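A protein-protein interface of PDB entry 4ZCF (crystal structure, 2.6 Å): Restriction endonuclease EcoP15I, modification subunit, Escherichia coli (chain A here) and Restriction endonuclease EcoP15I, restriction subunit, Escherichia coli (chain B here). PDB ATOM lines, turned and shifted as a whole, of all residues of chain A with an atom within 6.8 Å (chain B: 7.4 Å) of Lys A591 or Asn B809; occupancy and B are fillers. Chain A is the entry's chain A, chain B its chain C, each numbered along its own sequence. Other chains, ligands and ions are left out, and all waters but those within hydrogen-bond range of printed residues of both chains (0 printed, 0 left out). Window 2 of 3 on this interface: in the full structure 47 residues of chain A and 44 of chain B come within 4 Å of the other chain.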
ATOM      1  N   PHE A 585     -15.437  -4.690 -15.379  1.00  0.00           N
ATOM      2  CA  PHE A 585     -14.732  -4.295 -14.153  1.00  0.00           C
ATOM      3  C   PHE A 585     -14.842  -2.752 -14.078  1.00  0.00           C
ATOM      4  O   PHE A 585     -14.519  -2.062 -15.054  1.00  0.00           O
ATOM      5  CB  PHE A 585     -13.266  -4.789 -14.179  1.00  0.00           C
ATOM      6  CG  PHE A 585     -12.403  -4.373 -13.007  1.00  0.00           C
ATOM      7  CD1 PHE A 585     -12.447  -5.071 -11.807  1.00  0.00           C
ATOM      8  CD2 PHE A 585     -11.523  -3.299 -13.114  1.00  0.00           C
ATOM      9  CE1 PHE A 585     -11.639  -4.687 -10.723  1.00  0.00           C
ATOM     10  CE2 PHE A 585     -10.741  -2.896 -12.018  1.00  0.00           C
ATOM     11  CZ  PHE A 585     -10.809  -3.588 -10.831  1.00  0.00           C
ATOM     12  N   THR A 586     -15.374  -2.227 -12.959  1.00  0.00           N
ATOM     13  CA  THR A 586     -15.656  -0.800 -12.788  1.00  0.00           C
ATOM     14  C   THR A 586     -14.647  -0.043 -11.923  1.00  0.00           C
ATOM     15  O   THR A 586     -13.735  -0.645 -11.355  1.00  0.00           O
ATOM     16  CB  THR A 586     -17.072  -0.621 -12.239  1.00  0.00           C
ATOM     17  N   SER A 587     -14.816   1.295 -11.830  1.00  0.00           N
ATOM     18  CA  SER A 587     -14.007   2.179 -10.990  1.00  0.00           C
ATOM     19  C   SER A 587     -14.346   1.924  -9.518  1.00  0.00           C
ATOM     20  O   SER A 587     -13.520   2.188  -8.640  1.00  0.00           O
ATOM     21  CB  SER A 587     -14.278   3.636 -11.346  1.00  0.00           C
ATOM     22  OG  SER A 587     -13.863   3.899 -12.676  1.00  0.00           O
ATOM     23  N   GLU A 588     -15.573   1.405  -9.261  1.00  0.00           N
ATOM     24  CA  GLU A 588     -16.086   1.036  -7.935  1.00  0.00           C
ATOM     25  C   GLU A 588     -15.402  -0.246  -7.465  1.00  0.00           C
ATOM     26  O   GLU A 588     -15.024  -0.346  -6.294  1.00  0.00           O
ATOM     27  CB  GLU A 588     -17.629   0.862  -7.943  1.00  0.00           C
ATOM     28  CG  GLU A 588     -18.436   2.054  -8.451  1.00  0.00           C
ATOM     29  CD  GLU A 588     -17.944   3.448  -8.093  1.00  0.00           C
ATOM     30  OE1 GLU A 588     -17.779   3.736  -6.885  1.00  0.00           O
ATOM     31  OE2 GLU A 588     -17.735   4.256  -9.028  1.00  0.00           O
ATOM     32  N   ALA A 589     -15.229  -1.212  -8.398  1.00  0.00           N
ATOM     33  CA  ALA A 589     -14.560  -2.497  -8.195  1.00  0.00           C
ATOM     34  C   ALA A 589     -13.086  -2.271  -7.801  1.00  0.00           C
ATOM     35  O   ALA A 589     -12.603  -2.880  -6.844  1.00  0.00           O
ATOM     36  CB  ALA A 589     -14.665  -3.332  -9.461  1.00  0.00           C
ATOM     37  N   LEU A 590     -12.411  -1.329  -8.496  1.00  0.00           N
ATOM     38  CA  LEU A 590     -11.030  -0.900  -8.262  1.00  0.00           C
ATOM     39  C   LEU A 590     -10.879  -0.255  -6.879  1.00  0.00           C
ATOM     40  O   LEU A 590      -9.929  -0.592  -6.163  1.00  0.00           O
ATOM     41  CB  LEU A 590     -10.599   0.078  -9.381  1.00  0.00           C
ATOM     42  CG  LEU A 590      -9.151   0.592  -9.403  1.00  0.00           C
ATOM     43  CD1 LEU A 590      -8.131  -0.551  -9.475  1.00  0.00           C
ATOM     44  CD2 LEU A 590      -8.946   1.535 -10.566  1.00  0.00           C
ATOM     45  N   LYS A 591     -11.820   0.656  -6.499  1.00  0.00           N
ATOM     46  CA  LYS A 591     -11.835   1.321  -5.189  1.00  0.00           C
ATOM     47  C   LYS A 591     -12.093   0.309  -4.083  1.00  0.00           C
ATOM     48  O   LYS A 591     -11.524   0.444  -2.997  1.00  0.00           O
ATOM     49  CB  LYS A 591     -12.908   2.413  -5.133  1.00  0.00           C
ATOM     50  CG  LYS A 591     -12.353   3.841  -5.064  1.00  0.00           C
ATOM     51  CD  LYS A 591     -12.587   4.649  -6.365  1.00  0.00           C
ATOM     52  CE  LYS A 591     -14.045   4.945  -6.695  1.00  0.00           C
ATOM     53  NZ  LYS A 591     -14.712   5.796  -5.668  1.00  0.00           N
ATOM     54  N   ALA A 592     -12.953  -0.698  -4.355  1.00  0.00           N
ATOM     55  CA  ALA A 592     -13.272  -1.743  -3.385  1.00  0.00           C
ATOM     56  C   ALA A 592     -12.059  -2.663  -3.191  1.00  0.00           C
ATOM     57  O   ALA A 592     -11.804  -3.101  -2.068  1.00  0.00           O
ATOM     58  CB  ALA A 592     -14.489  -2.535  -3.834  1.00  0.00           C
ATOM     59  N   LEU A 593     -11.293  -2.913  -4.284  1.00  0.00           N
ATOM     60  CA  LEU A 593     -10.057  -3.697  -4.295  1.00  0.00           C
ATOM     61  C   LEU A 593      -9.022  -3.037  -3.376  1.00  0.00           C
ATOM     62  O   LEU A 593      -8.482  -3.718  -2.509  1.00  0.00           O
ATOM     63  CB  LEU A 593      -9.544  -3.834  -5.744  1.00  0.00           C
ATOM     64  CG  LEU A 593      -8.153  -4.413  -6.050  1.00  0.00           C
ATOM     65  CD1 LEU A 593      -7.834  -5.669  -5.220  1.00  0.00           C
ATOM     66  CD2 LEU A 593      -8.065  -4.792  -7.513  1.00  0.00           C
ATOM     67  N   LEU A 594      -8.802  -1.711  -3.529  1.00  0.00           N
ATOM     68  CA  LEU A 594      -7.873  -0.924  -2.710  1.00  0.00           C
ATOM     69  C   LEU A 594      -8.363  -0.836  -1.257  1.00  0.00           C
ATOM     70  O   LEU A 594      -7.551  -0.864  -0.334  1.00  0.00           O
ATOM     71  CB  LEU A 594      -7.638   0.479  -3.311  1.00  0.00           C
ATOM     72  CG  LEU A 594      -7.193   0.553  -4.797  1.00  0.00           C
ATOM     73  CD1 LEU A 594      -7.470   1.912  -5.373  1.00  0.00           C
ATOM     74  CD2 LEU A 594      -5.722   0.189  -4.986  1.00  0.00           C
ATOM     75  N   GLN A 595      -9.691  -0.791  -1.059  1.00  0.00           N
ATOM     76  CA  GLN A 595     -10.328  -0.784   0.261  1.00  0.00           C
ATOM     77  C   GLN A 595     -10.106  -2.136   0.975  1.00  0.00           C
ATOM     78  O   GLN A 595      -9.712  -2.141   2.142  1.00  0.00           O
ATOM     79  CB  GLN A 595     -11.820  -0.503   0.119  1.00  0.00           C
ATOM     80  N   LYS A 596     -10.320  -3.273   0.259  1.00  0.00           N
ATOM     81  CA  LYS A 596     -10.135  -4.642   0.761  1.00  0.00           C
ATOM     82  C   LYS A 596      -8.678  -4.911   1.135  1.00  0.00           C
ATOM     83  O   LYS A 596      -8.430  -5.687   2.063  1.00  0.00           O
ATOM     84  CB  LYS A 596     -10.670  -5.691  -0.233  1.00  0.00           C
ATOM     85  CG  LYS A 596     -11.092  -6.999   0.443  1.00  0.00           C
ATOM     86  CD  LYS A 596     -11.888  -7.914  -0.485  1.00  0.00           C
ATOM     87  CE  LYS A 596     -12.647  -8.976   0.279  1.00  0.00           C
ATOM     88  NZ  LYS A 596     -13.914  -9.362  -0.411  1.00  0.00           N
ATOM     89  N   GLN B 677      -5.534  13.761   1.214  1.00  0.00           N
ATOM     90  CA  GLN B 677      -6.721  13.065   0.702  1.00  0.00           C
ATOM     91  C   GLN B 677      -6.392  12.385  -0.633  1.00  0.00           C
ATOM     92  O   GLN B 677      -6.096  13.064  -1.621  1.00  0.00           O
ATOM     93  CB  GLN B 677      -7.878  14.037   0.544  1.00  0.00           C
ATOM     94  N   LYS B 678      -6.395  11.035  -0.637  1.00  0.00           N
ATOM     95  CA  LYS B 678      -6.054  10.193  -1.791  1.00  0.00           C
ATOM     96  C   LYS B 678      -7.179  10.039  -2.816  1.00  0.00           C
ATOM     97  O   LYS B 678      -8.362   9.995  -2.459  1.00  0.00           O
ATOM     98  CB  LYS B 678      -5.569   8.826  -1.326  1.00  0.00           C
ATOM     99  N   ALA B 679      -6.784   9.963  -4.100  1.00  0.00           N
ATOM    100  CA  ALA B 679      -7.669   9.809  -5.253  1.00  0.00           C
ATOM    101  C   ALA B 679      -7.092   8.795  -6.243  1.00  0.00           C
ATOM    102  O   ALA B 679      -5.904   8.450  -6.154  1.00  0.00           O
ATOM    103  CB  ALA B 679      -7.869  11.152  -5.941  1.00  0.00           C
ATOM    104  N   VAL B 680      -7.936   8.327  -7.190  1.00  0.00           N
ATOM    105  CA  VAL B 680      -7.552   7.360  -8.219  1.00  0.00           C
ATOM    106  C   VAL B 680      -7.951   7.800  -9.631  1.00  0.00           C
ATOM    107  O   VAL B 680      -9.115   8.107  -9.896  1.00  0.00           O
ATOM    108  CB  VAL B 680      -7.958   5.910  -7.836  1.00  0.00           C
ATOM    109  CG1 VAL B 680      -8.317   5.052  -9.050  1.00  0.00           C
ATOM    110  CG2 VAL B 680      -6.860   5.251  -7.013  1.00  0.00           C
ATOM    111  N   GLU B 682      -8.884   7.962 -13.529  1.00  0.00           N
ATOM    112  CA  GLU B 682      -9.892   7.329 -14.370  1.00  0.00           C
ATOM    113  C   GLU B 682      -9.779   7.961 -15.750  1.00  0.00           C
ATOM    114  O   GLU B 682      -9.737   9.188 -15.867  1.00  0.00           O
ATOM    115  CB  GLU B 682     -11.306   7.504 -13.801  1.00  0.00           C
ATOM    116  CG  GLU B 682     -12.369   6.764 -14.608  1.00  0.00           C
ATOM    117  CD  GLU B 682     -13.799   6.828 -14.101  1.00  0.00           C
ATOM    118  OE1 GLU B 682     -14.065   7.556 -13.117  1.00  0.00           O
ATOM    119  OE2 GLU B 682     -14.661   6.150 -14.705  1.00  0.00           O
ATOM    120  N   GLY B 807     -10.266  11.763 -11.598  1.00  0.00           N
ATOM    121  CA  GLY B 807      -9.763  11.406 -10.278  1.00  0.00           C
ATOM    122  C   GLY B 807     -10.981  11.031  -9.427  1.00  0.00           C
ATOM    123  O   GLY B 807     -11.854  11.868  -9.216  1.00  0.00           O
ATOM    124  N   TYR B 808     -11.066   9.758  -9.005  1.00  0.00           N
ATOM    125  CA  TYR B 808     -12.136   9.218  -8.167  1.00  0.00           C
ATOM    126  C   TYR B 808     -11.631   9.116  -6.718  1.00  0.00           C
ATOM    127  O   TYR B 808     -10.535   8.595  -6.481  1.00  0.00           O
ATOM    128  CB  TYR B 808     -12.570   7.854  -8.681  1.00  0.00           C
ATOM    129  N   ASN B 809     -12.426   9.646  -5.759  1.00  0.00           N
ATOM    130  CA  ASN B 809     -12.104   9.710  -4.328  1.00  0.00           C
ATOM    131  C   ASN B 809     -11.949   8.352  -3.619  1.00  0.00           C
ATOM    132  O   ASN B 809     -12.942   7.683  -3.300  1.00  0.00           O
ATOM    133  CB  ASN B 809     -13.098  10.602  -3.597  1.00  0.00           C
ATOM    134  N   LEU B 810     -10.675   7.969  -3.366  1.00  0.00           N
ATOM    135  CA  LEU B 810     -10.279   6.724  -2.712  1.00  0.00           C
ATOM    136  C   LEU B 810      -9.616   7.012  -1.381  1.00  0.00           C
ATOM    137  O   LEU B 810      -9.979   6.404  -0.379  1.00  0.00           O
ATOM    138  CB  LEU B 810      -9.327   5.944  -3.606  1.00  0.00           C
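OE1 of Glu A588 lies within salt-bridge range of NZ of Lys A591 (3.9 Å).
The backbone carbonyl oxygen of Lys B678 lies within hydrogen-bond range of the backbone NH of Leu B810, at 3.2 Å.
N of Tyr B808 lies within hydrogen-bond range of O of Val B680 (2.7 Å).
Hydrophobic or aromatic side chains of chain B within 4 Å of the printed part of chain A: Val B680, Tyr B808 and Leu B810.
Of the 12 printed residues of chain A, 4 touch a printed residue of chain B.
Among the printed residues, no Asp or Glu carboxylate lies within 4 Å of a Lys or Arg side-chain nitrogen of the other chain.
Lys A591 touches just these residues of chain B: Tyr B808, Asn B809 and Leu B810.
Leu A593 touches none of the printed residues of chain B.
Of the printed residues of chain B, Leu A594 touches Val B680 (3.8 Å).
Lys A596 touches none of the printed residues of chain B.
Printed residues of chain A within 4 Å of Val B680: Leu A590 and Leu A594.
Of the printed residues of chain A, Glu B682 touches Ser A587 (3.1 Å).
Of the printed residues of chain A, Tyr B808 touches Lys A591 (3.8 Å).
Of chain A, only Lys A591 (3.5 Å) comes within 4 Å of Asn B809.
Printed residues of chain A within 4 Å of Leu B810: Lys A591 (3.96 Å).
The side-chain hydroxyl (OG) of Ser A587 is in hydrogen-bond range of the side-chain carboxylate (OE2) of Glu B682, at 3.1 Å.
Among the printed residues, pairs that only touch across the chains: Lys A591 with Asn B809 (3.5 Å), Leu A594 with Val B680 (3.8 Å), Lys A591 with Tyr B808 (3.8 Å), Leu A590 with Val B680 (3.9 Å) and Lys A591 with Leu B810 (3.96 Å).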
